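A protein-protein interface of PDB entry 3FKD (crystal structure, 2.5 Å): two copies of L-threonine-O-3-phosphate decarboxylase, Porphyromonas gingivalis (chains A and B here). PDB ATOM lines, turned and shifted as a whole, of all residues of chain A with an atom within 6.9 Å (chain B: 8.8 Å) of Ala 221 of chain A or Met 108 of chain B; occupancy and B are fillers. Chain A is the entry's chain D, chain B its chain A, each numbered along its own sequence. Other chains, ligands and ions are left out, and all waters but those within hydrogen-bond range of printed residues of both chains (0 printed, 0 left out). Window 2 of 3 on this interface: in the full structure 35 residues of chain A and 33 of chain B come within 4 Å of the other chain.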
ATOM      1  N   GLN A  82       3.641  21.649 -22.227  1.00  0.00           N
ATOM      2  CA  GLN A  82       2.655  21.059 -21.354  1.00  0.00           C
ATOM      3  C   GLN A  82       3.284  20.530 -20.041  1.00  0.00           C
ATOM      4  O   GLN A  82       2.670  20.554 -18.986  1.00  0.00           O
ATOM      5  CB  GLN A  82       1.855  20.009 -22.069  1.00  0.00           C
ATOM      6  CG  GLN A  82       0.467  19.861 -21.484  1.00  0.00           C
ATOM      7  CD  GLN A  82      -0.276  18.650 -22.028  1.00  0.00           C
ATOM      8  OE1 GLN A  82      -0.926  17.913 -21.275  1.00  0.00           O
ATOM      9  NE2 GLN A  82      -0.166  18.426 -23.339  1.00  0.00           N
ATOM     10  N   GLN A  85       4.006  23.504 -17.827  1.00  0.00           N
ATOM     11  CA  GLN A  85       2.783  24.102 -17.345  1.00  0.00           C
ATOM     12  C   GLN A  85       2.237  23.330 -16.146  1.00  0.00           C
ATOM     13  O   GLN A  85       1.680  23.919 -15.223  1.00  0.00           O
ATOM     14  CB  GLN A  85       1.779  24.225 -18.497  1.00  0.00           C
ATOM     15  CG  GLN A  85       0.301  24.275 -18.086  1.00  0.00           C
ATOM     16  CD  GLN A  85      -0.667  24.264 -19.280  1.00  0.00           C
ATOM     17  OE1 GLN A  85      -0.519  23.485 -20.235  1.00  0.00           O
ATOM     18  NE2 GLN A  85      -1.668  25.129 -19.216  1.00  0.00           N
ATOM     19  N   ALA A  86       2.432  22.019 -16.162  1.00  0.00           N
ATOM     20  CA  ALA A  86       1.917  21.135 -15.130  1.00  0.00           C
ATOM     21  C   ALA A  86       2.683  21.304 -13.787  1.00  0.00           C
ATOM     22  O   ALA A  86       2.214  20.881 -12.712  1.00  0.00           O
ATOM     23  CB  ALA A  86       1.965  19.683 -15.621  1.00  0.00           C
ATOM     24  N   MET A 216       2.562  11.809 -15.196  1.00  0.00           N
ATOM     25  CA  MET A 216       1.619  11.896 -16.294  1.00  0.00           C
ATOM     26  C   MET A 216       0.240  12.420 -15.881  1.00  0.00           C
ATOM     27  O   MET A 216      -0.403  13.136 -16.646  1.00  0.00           O
ATOM     28  CB  MET A 216       1.446  10.540 -16.978  1.00  0.00           C
ATOM     29  CG  MET A 216       0.764  10.675 -18.322  1.00  0.00           C
ATOM     30  SD  MET A 216       1.977  11.580 -19.555  1.00  0.00           S
ATOM     31  CE  MET A 216       3.053  10.068 -20.136  1.00  0.00           C
ATOM     32  N   LYS A 217      -0.212  12.044 -14.685  1.00  0.00           N
ATOM     33  CA  LYS A 217      -1.473  12.523 -14.163  1.00  0.00           C
ATOM     34  C   LYS A 217      -1.447  14.045 -14.088  1.00  0.00           C
ATOM     35  O   LYS A 217      -2.406  14.726 -14.471  1.00  0.00           O
ATOM     36  CB  LYS A 217      -1.730  11.932 -12.775  1.00  0.00           C
ATOM     37  CG  LYS A 217      -3.178  11.902 -12.364  1.00  0.00           C
ATOM     38  CD  LYS A 217      -3.958  10.955 -13.288  1.00  0.00           C
ATOM     39  CE  LYS A 217      -5.176  10.344 -12.556  1.00  0.00           C
ATOM     40  NZ  LYS A 217      -5.555   8.976 -13.056  1.00  0.00           N
ATOM     41  N   ARG A 218      -0.345  14.575 -13.596  1.00  0.00           N
ATOM     42  CA  ARG A 218      -0.158  16.014 -13.480  1.00  0.00           C
ATOM     43  C   ARG A 218      -0.090  16.686 -14.872  1.00  0.00           C
ATOM     44  O   ARG A 218      -0.605  17.787 -15.082  1.00  0.00           O
ATOM     45  CB  ARG A 218       1.121  16.281 -12.698  1.00  0.00           C
ATOM     46  CG  ARG A 218       1.101  17.570 -11.920  1.00  0.00           C
ATOM     47  CD  ARG A 218       0.814  17.350 -10.428  1.00  0.00           C
ATOM     48  NE  ARG A 218       0.608  18.642  -9.778  1.00  0.00           N
ATOM     49  CZ  ARG A 218       1.583  19.527  -9.600  1.00  0.00           C
ATOM     50  NH1 ARG A 218       2.818  19.220 -10.000  1.00  0.00           N
ATOM     51  NH2 ARG A 218       1.343  20.697  -9.005  1.00  0.00           N
ATOM     52  N   VAL A 219       0.539  16.017 -15.825  1.00  0.00           N
ATOM     53  CA  VAL A 219       0.552  16.505 -17.201  1.00  0.00           C
ATOM     54  C   VAL A 219      -0.844  16.471 -17.841  1.00  0.00           C
ATOM     55  O   VAL A 219      -1.287  17.445 -18.424  1.00  0.00           O
ATOM     56  CB  VAL A 219       1.534  15.687 -18.049  1.00  0.00           C
ATOM     57  CG1 VAL A 219       1.570  16.193 -19.472  1.00  0.00           C
ATOM     58  CG2 VAL A 219       2.881  15.749 -17.415  1.00  0.00           C
ATOM     59  N   ALA A 220      -1.511  15.326 -17.699  1.00  0.00           N
ATOM     60  CA  ALA A 220      -2.806  15.043 -18.307  1.00  0.00           C
ATOM     61  C   ALA A 220      -3.868  16.092 -17.976  1.00  0.00           C
ATOM     62  O   ALA A 220      -4.714  16.369 -18.802  1.00  0.00           O
ATOM     63  CB  ALA A 220      -3.274  13.651 -17.908  1.00  0.00           C
ATOM     64  N   ALA A 221      -3.813  16.681 -16.782  1.00  0.00           N
ATOM     65  CA  ALA A 221      -4.797  17.685 -16.350  1.00  0.00           C
ATOM     66  C   ALA A 221      -4.879  18.880 -17.300  1.00  0.00           C
ATOM     67  O   ALA A 221      -5.821  19.674 -17.238  1.00  0.00           O
ATOM     68  CB  ALA A 221      -4.503  18.166 -14.943  1.00  0.00           C
ATOM     69  N   PHE A 222      -3.911  19.011 -18.195  1.00  0.00           N
ATOM     70  CA  PHE A 222      -3.943  20.139 -19.107  1.00  0.00           C
ATOM     71  C   PHE A 222      -4.069  19.712 -20.565  1.00  0.00           C
ATOM     72  O   PHE A 222      -3.906  20.541 -21.463  1.00  0.00           O
ATOM     73  CB  PHE A 222      -2.714  21.048 -18.896  1.00  0.00           C
ATOM     74  CG  PHE A 222      -2.655  21.693 -17.535  1.00  0.00           C
ATOM     75  CD1 PHE A 222      -3.293  22.906 -17.292  1.00  0.00           C
ATOM     76  CD2 PHE A 222      -1.946  21.096 -16.492  1.00  0.00           C
ATOM     77  CE1 PHE A 222      -3.283  23.493 -16.014  1.00  0.00           C
ATOM     78  CE2 PHE A 222      -1.918  21.690 -15.208  1.00  0.00           C
ATOM     79  CZ  PHE A 222      -2.588  22.877 -14.976  1.00  0.00           C
ATOM     80  N   SER A 223      -4.311  18.424 -20.807  1.00  0.00           N
ATOM     81  CA  SER A 223      -4.626  17.937 -22.162  1.00  0.00           C
ATOM     82  C   SER A 223      -5.952  18.478 -22.700  1.00  0.00           C
ATOM     83  O   SER A 223      -6.972  18.493 -21.997  1.00  0.00           O
ATOM     84  CB  SER A 223      -4.737  16.410 -22.209  1.00  0.00           C
ATOM     85  OG  SER A 223      -3.644  15.809 -21.578  1.00  0.00           O
ATOM     86  N   THR A 224      -5.938  18.855 -23.968  1.00  0.00           N
ATOM     87  CA  THR A 224      -7.137  19.333 -24.644  1.00  0.00           C
ATOM     88  C   THR A 224      -7.565  18.368 -25.748  1.00  0.00           C
ATOM     89  O   THR A 224      -6.742  17.728 -26.363  1.00  0.00           O
ATOM     90  CB  THR A 224      -6.915  20.762 -25.180  1.00  0.00           C
ATOM     91  OG1 THR A 224      -6.041  20.723 -26.312  1.00  0.00           O
ATOM     92  CG2 THR A 224      -6.315  21.670 -24.063  1.00  0.00           C
ATOM     93  N   PHE B  80     -10.476  28.153 -27.483  1.00  0.00           N
ATOM     94  CA  PHE B  80     -11.340  28.352 -26.311  1.00  0.00           C
ATOM     95  C   PHE B  80     -10.515  28.218 -25.040  1.00  0.00           C
ATOM     96  O   PHE B  80     -10.666  28.984 -24.097  1.00  0.00           O
ATOM     97  CB  PHE B  80     -12.500  27.348 -26.281  1.00  0.00           C
ATOM     98  CG  PHE B  80     -13.433  27.497 -27.414  1.00  0.00           C
ATOM     99  CD1 PHE B  80     -13.928  28.747 -27.754  1.00  0.00           C
ATOM    100  CD2 PHE B  80     -13.816  26.402 -28.154  1.00  0.00           C
ATOM    101  CE1 PHE B  80     -14.766  28.892 -28.800  1.00  0.00           C
ATOM    102  CE2 PHE B  80     -14.675  26.537 -29.201  1.00  0.00           C
ATOM    103  CZ  PHE B  80     -15.149  27.776 -29.526  1.00  0.00           C
ATOM    104  N   TYR B  81      -9.651  27.213 -25.062  1.00  0.00           N
ATOM    105  CA  TYR B  81      -8.673  26.942 -24.046  1.00  0.00           C
ATOM    106  C   TYR B  81      -7.591  28.039 -23.942  1.00  0.00           C
ATOM    107  O   TYR B  81      -7.201  28.444 -22.837  1.00  0.00           O
ATOM    108  CB  TYR B  81      -8.048  25.608 -24.397  1.00  0.00           C
ATOM    109  CG  TYR B  81      -8.895  24.440 -23.987  1.00  0.00           C
ATOM    110  CD1 TYR B  81      -8.803  23.901 -22.695  1.00  0.00           C
ATOM    111  CD2 TYR B  81      -9.814  23.888 -24.854  1.00  0.00           C
ATOM    112  CE1 TYR B  81      -9.586  22.835 -22.303  1.00  0.00           C
ATOM    113  CE2 TYR B  81     -10.578  22.804 -24.477  1.00  0.00           C
ATOM    114  CZ  TYR B  81     -10.453  22.290 -23.197  1.00  0.00           C
ATOM    115  OH  TYR B  81     -11.229  21.225 -22.827  1.00  0.00           O
ATOM    116  N   GLN B  82      -7.072  28.507 -25.077  1.00  0.00           N
ATOM    117  CA  GLN B  82      -6.085  29.554 -24.975  1.00  0.00           C
ATOM    118  C   GLN B  82      -6.669  30.841 -24.375  1.00  0.00           C
ATOM    119  O   GLN B  82      -5.947  31.611 -23.733  1.00  0.00           O
ATOM    120  CB  GLN B  82      -5.408  29.837 -26.315  1.00  0.00           C
ATOM    121  CG  GLN B  82      -3.898  30.094 -26.167  1.00  0.00           C
ATOM    122  CD  GLN B  82      -3.288  30.802 -27.361  1.00  0.00           C
ATOM    123  OE1 GLN B  82      -3.358  30.326 -28.496  1.00  0.00           O
ATOM    124  NE2 GLN B  82      -2.682  31.948 -27.111  1.00  0.00           N
ATOM    125  N   ALA B  84      -9.473  31.007 -22.187  1.00  0.00           N
ATOM    126  CA  ALA B  84      -9.605  30.599 -20.792  1.00  0.00           C
ATOM    127  C   ALA B  84      -8.298  30.765 -20.052  1.00  0.00           C
ATOM    128  O   ALA B  84      -8.282  31.394 -18.999  1.00  0.00           O
ATOM    129  CB  ALA B  84     -10.053  29.169 -20.697  1.00  0.00           C
ATOM    130  N   GLN B  85      -7.213  30.220 -20.620  1.00  0.00           N
ATOM    131  CA  GLN B  85      -5.864  30.330 -20.052  1.00  0.00           C
ATOM    132  C   GLN B  85      -5.436  31.766 -19.769  1.00  0.00           C
ATOM    133  O   GLN B  85      -5.058  32.112 -18.607  1.00  0.00           O
ATOM    134  CB  GLN B  85      -4.813  29.612 -20.911  1.00  0.00           C
ATOM    135  CG  GLN B  85      -3.534  29.271 -20.163  1.00  0.00           C
ATOM    136  CD  GLN B  85      -2.434  28.666 -21.048  1.00  0.00           C
ATOM    137  OE1 GLN B  85      -2.603  28.508 -22.258  1.00  0.00           O
ATOM    138  NE2 GLN B  85      -1.300  28.346 -20.443  1.00  0.00           N
ATOM    139  N   ARG B  88      -7.248  33.163 -16.473  1.00  0.00           N
ATOM    140  CA  ARG B  88      -7.399  32.222 -15.356  1.00  0.00           C
ATOM    141  C   ARG B  88      -8.184  32.740 -14.152  1.00  0.00           C
ATOM    142  O   ARG B  88      -8.939  32.000 -13.515  1.00  0.00           O
ATOM    143  CB  ARG B  88      -6.035  31.744 -14.854  1.00  0.00           C
ATOM    144  CG  ARG B  88      -6.074  31.130 -13.466  1.00  0.00           C
ATOM    145  CD  ARG B  88      -4.918  30.172 -13.313  1.00  0.00           C
ATOM    146  NE  ARG B  88      -4.988  29.290 -12.143  1.00  0.00           N
ATOM    147  CZ  ARG B  88      -3.912  28.705 -11.592  1.00  0.00           C
ATOM    148  NH1 ARG B  88      -2.702  28.931 -12.097  1.00  0.00           N
ATOM    149  NH2 ARG B  88      -4.021  27.907 -10.529  1.00  0.00           N
ATOM    150  N   GLU B 101     -17.049  22.258 -24.451  1.00  0.00           N
ATOM    151  CA  GLU B 101     -15.707  22.779 -24.425  1.00  0.00           C
ATOM    152  C   GLU B 101     -15.565  24.196 -23.874  1.00  0.00           C
ATOM    153  O   GLU B 101     -14.480  24.551 -23.423  1.00  0.00           O
ATOM    154  CB  GLU B 101     -15.070  22.616 -25.806  1.00  0.00           C
ATOM    155  CG  GLU B 101     -15.063  21.141 -26.270  1.00  0.00           C
ATOM    156  CD  GLU B 101     -14.205  20.259 -25.385  1.00  0.00           C
ATOM    157  OE1 GLU B 101     -13.216  20.769 -24.804  1.00  0.00           O
ATOM    158  OE2 GLU B 101     -14.529  19.052 -25.275  1.00  0.00           O
ATOM    159  N   TYR B 102     -16.614  25.013 -23.900  1.00  0.00           N
ATOM    160  CA  TYR B 102     -16.523  26.290 -23.199  1.00  0.00           C
ATOM    161  C   TYR B 102     -16.356  25.998 -21.717  1.00  0.00           C
ATOM    162  O   TYR B 102     -15.468  26.557 -21.055  1.00  0.00           O
ATOM    163  CB  TYR B 102     -17.720  27.216 -23.420  1.00  0.00           C
ATOM    164  CG  TYR B 102     -18.262  27.250 -24.823  1.00  0.00           C
ATOM    165  CD1 TYR B 102     -17.407  27.143 -25.942  1.00  0.00           C
ATOM    166  CD2 TYR B 102     -19.643  27.401 -25.045  1.00  0.00           C
ATOM    167  CE1 TYR B 102     -17.928  27.182 -27.242  1.00  0.00           C
ATOM    168  CE2 TYR B 102     -20.172  27.431 -26.323  1.00  0.00           C
ATOM    169  CZ  TYR B 102     -19.313  27.315 -27.435  1.00  0.00           C
ATOM    170  OH  TYR B 102     -19.845  27.342 -28.707  1.00  0.00           O
ATOM    171  N   GLU B 103     -17.184  25.084 -21.217  1.00  0.00           N
ATOM    172  CA  GLU B 103     -17.123  24.716 -19.818  1.00  0.00           C
ATOM    173  C   GLU B 103     -15.751  24.137 -19.447  1.00  0.00           C
ATOM    174  O   GLU B 103     -15.124  24.602 -18.503  1.00  0.00           O
ATOM    175  CB  GLU B 103     -18.217  23.728 -19.454  1.00  0.00           C
ATOM    176  CG  GLU B 103     -18.640  23.817 -18.005  1.00  0.00           C
ATOM    177  CD  GLU B 103     -19.481  22.614 -17.537  1.00  0.00           C
ATOM    178  OE1 GLU B 103     -20.504  22.283 -18.182  1.00  0.00           O
ATOM    179  OE2 GLU B 103     -19.109  21.999 -16.500  1.00  0.00           O
ATOM    180  N   ASP B 104     -15.306  23.127 -20.194  1.00  0.00           N
ATOM    181  CA  ASP B 104     -14.081  22.420 -19.875  1.00  0.00           C
ATOM    182  C   ASP B 104     -12.931  23.387 -19.836  1.00  0.00           C
ATOM    183  O   ASP B 104     -12.101  23.298 -18.949  1.00  0.00           O
ATOM    184  CB  ASP B 104     -13.786  21.309 -20.879  1.00  0.00           C
ATOM    185  CG  ASP B 104     -14.866  20.250 -20.914  1.00  0.00           C
ATOM    186  OD1 ASP B 104     -15.538  20.039 -19.864  1.00  0.00           O
ATOM    187  OD2 ASP B 104     -15.054  19.629 -21.991  1.00  0.00           O
ATOM    188  N   ALA B 105     -12.908  24.329 -20.778  1.00  0.00           N
ATOM    189  CA  ALA B 105     -11.863  25.356 -20.784  1.00  0.00           C
ATOM    190  C   ALA B 105     -11.855  26.186 -19.512  1.00  0.00           C
ATOM    191  O   ALA B 105     -10.813  26.356 -18.873  1.00  0.00           O
ATOM    192  CB  ALA B 105     -11.971  26.269 -22.003  1.00  0.00           C
ATOM    193  N   CYS B 106     -13.019  26.731 -19.199  1.00  0.00           N
ATOM    194  CA  CYS B 106     -13.218  27.591 -18.054  1.00  0.00           C
ATOM    195  C   CYS B 106     -12.854  26.867 -16.753  1.00  0.00           C
ATOM    196  O   CYS B 106     -12.372  27.480 -15.809  1.00  0.00           O
ATOM    197  CB  CYS B 106     -14.672  28.049 -18.004  1.00  0.00           C
ATOM    198  SG  CYS B 106     -15.049  29.519 -19.002  1.00  0.00           S
ATOM    199  N   ARG B 107     -13.116  25.567 -16.693  1.00  0.00           N
ATOM    200  CA  ARG B 107     -12.827  24.801 -15.495  1.00  0.00           C
ATOM    201  C   ARG B 107     -11.315  24.594 -15.426  1.00  0.00           C
ATOM    202  O   ARG B 107     -10.680  24.912 -14.424  1.00  0.00           O
ATOM    203  CB  ARG B 107     -13.577  23.457 -15.482  1.00  0.00           C
ATOM    204  CG  ARG B 107     -13.012  22.455 -14.456  1.00  0.00           C
ATOM    205  CD  ARG B 107     -13.548  21.058 -14.613  1.00  0.00           C
ATOM    206  NE  ARG B 107     -13.145  20.513 -15.910  1.00  0.00           N
ATOM    207  CZ  ARG B 107     -13.454  19.295 -16.374  1.00  0.00           C
ATOM    208  NH1 ARG B 107     -14.169  18.446 -15.637  1.00  0.00           N
ATOM    209  NH2 ARG B 107     -13.028  18.920 -17.585  1.00  0.00           N
ATOM    210  N   MET B 108     -10.737  24.079 -16.506  1.00  0.00           N
ATOM    211  CA  MET B 108      -9.324  23.776 -16.482  1.00  0.00           C
ATOM    212  C   MET B 108      -8.576  24.981 -15.984  1.00  0.00           C
ATOM    213  O   MET B 108      -7.630  24.850 -15.212  1.00  0.00           O
ATOM    214  CB  MET B 108      -8.821  23.341 -17.850  1.00  0.00           C
ATOM    215  CG  MET B 108      -7.316  23.252 -17.958  1.00  0.00           C
ATOM    216  SD  MET B 108      -6.819  22.608 -19.731  1.00  0.00           S
ATOM    217  CE  MET B 108      -4.959  23.184 -19.765  1.00  0.00           C
ATOM    218  N   TYR B 109      -9.014  26.170 -16.382  1.00  0.00           N
ATOM    219  CA  TYR B 109      -8.308  27.363 -15.927  1.00  0.00           C
ATOM    220  C   TYR B 109      -8.966  28.074 -14.727  1.00  0.00           C
ATOM    221  O   TYR B 109      -8.717  29.250 -14.463  1.00  0.00           O
ATOM    222  CB  TYR B 109      -7.950  28.273 -17.107  1.00  0.00           C
ATOM    223  CG  TYR B 109      -6.979  27.552 -18.007  1.00  0.00           C
ATOM    224  CD1 TYR B 109      -7.425  26.844 -19.120  1.00  0.00           C
ATOM    225  CD2 TYR B 109      -5.626  27.511 -17.710  1.00  0.00           C
ATOM    226  CE1 TYR B 109      -6.558  26.150 -19.916  1.00  0.00           C
ATOM    227  CE2 TYR B 109      -4.729  26.817 -18.514  1.00  0.00           C
ATOM    228  CZ  TYR B 109      -5.206  26.141 -19.623  1.00  0.00           C
ATOM    229  OH  TYR B 109      -4.343  25.453 -20.431  1.00  0.00           O
ATOM    230  N   GLU B 110      -9.758  27.305 -13.984  1.00  0.00           N
ATOM    231  CA  GLU B 110     -10.384  27.734 -12.723  1.00  0.00           C
ATOM    232  C   GLU B 110     -11.121  29.086 -12.775  1.00  0.00           C
ATOM    233  O   GLU B 110     -10.921  29.956 -11.928  1.00  0.00           O
ATOM    234  CB  GLU B 110      -9.370  27.675 -11.574  1.00  0.00           C
ATOM    235  CG  GLU B 110      -8.987  26.249 -11.157  1.00  0.00           C
ATOM    236  CD  GLU B 110      -7.539  26.134 -10.605  1.00  0.00           C
ATOM    237  OE1 GLU B 110      -6.832  27.180 -10.502  1.00  0.00           O
ATOM    238  OE2 GLU B 110      -7.114  24.989 -10.281  1.00  0.00           O
ATOM    239  N   HIS B 111     -11.945  29.240 -13.813  1.00  0.00           N
ATOM    240  CA  HIS B 111     -12.954  30.281 -13.920  1.00  0.00           C
ATOM    241  C   HIS B 111     -14.071  29.937 -12.930  1.00  0.00           C
ATOM    242  O   HIS B 111     -14.355  28.763 -12.699  1.00  0.00           O
ATOM    243  CB  HIS B 111     -13.538  30.290 -15.353  1.00  0.00           C
ATOM    244  CG  HIS B 111     -12.743  31.085 -16.355  1.00  0.00           C
ATOM    245  ND1 HIS B 111     -11.430  30.794 -16.683  1.00  0.00           N
ATOM    246  CD2 HIS B 111     -13.089  32.152 -17.119  1.00  0.00           C
ATOM    247  CE1 HIS B 111     -11.002  31.652 -17.592  1.00  0.00           C
ATOM    248  NE2 HIS B 111     -11.987  32.485 -17.871  1.00  0.00           N
ATOM    249  N   VAL B 113     -17.765  29.584 -12.856  1.00  0.00           N
ATOM    250  CA  VAL B 113     -18.725  29.410 -13.930  1.00  0.00           C
ATOM    251  C   VAL B 113     -20.230  29.497 -13.541  1.00  0.00           C
ATOM    252  O   VAL B 113     -20.750  28.667 -12.800  1.00  0.00           O
ATOM    253  CB  VAL B 113     -18.413  28.105 -14.742  1.00  0.00           C
ATOM    254  CG1 VAL B 113     -19.402  27.928 -15.884  1.00  0.00           C
ATOM    255  CG2 VAL B 113     -17.018  28.175 -15.317  1.00  0.00           C
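NE2 of Gln 85 of chain B sits close to NE2 of Gln 85 of chain A. The side-chain hydroxyl (OH) of Tyr 109 of chain B is in hydrogen-bond range of the side-chain amide nitrogen (NE2) of Gln 85 of chain A (3.0 Å).
The side-chain hydroxyl of Tyr 81 of chain B sits at hydrogen-bond distance from the side-chain carboxylate of Glu 101 of chain B.
Among the printed residues, pairs that only touch across the chains: Gln 85 of chain A with Met 108 of chain B (3.9 Å), Ala 221 of chain A with Met 108 of chain B (3.9 Å), Phe 222 of chain A with Met 108 of chain B (3.0 Å) and Thr 224 of chain A with Tyr 81 of chain B (3.6 Å).
Of chain B, only Met 108 comes within 4 Å of Ala 221 of chain A. Met 108 of chain B touches just these residues of chain A: Gln 85, Ala 221 and Phe 222. No residue of chain B comes within 4 Å of Ala 220 of chain A. Of the printed residues of chain A, Tyr 109 of chain B touches Gln 85. Of the printed residues of chain A, Gln 85 of chain B touches Gln 85. Printed residues of chain B within 4 Å of Phe 222 of chain A: Met 108 (3.0 Å). Of the printed residues of chain B, Thr 224 of chain A touches Tyr 81. Tyr 102 of chain B touches none of the printed residues of chain A. Val 113 of chain B touches none of the printed residues of chain A. The nearest residue of chain A that does not touch Met 108 of chain B is Thr 224 of chain A (4.5 Å).
Of the 12 printed residues of chain A, 4 touch a printed residue of chain B. Hydrophobic or aromatic side chains of chain B within 4 Å of the printed part of chain A: Tyr 81, Met 108 and Tyr 109. Among the printed residues, no Asp or Glu carboxylate lies within 4 Å of a Lys or Arg side-chain nitrogen of the other chain.
Gln 85 of chain B touches its own counterpart, Gln 85 of chain A. 2 positions are printed for both chains.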
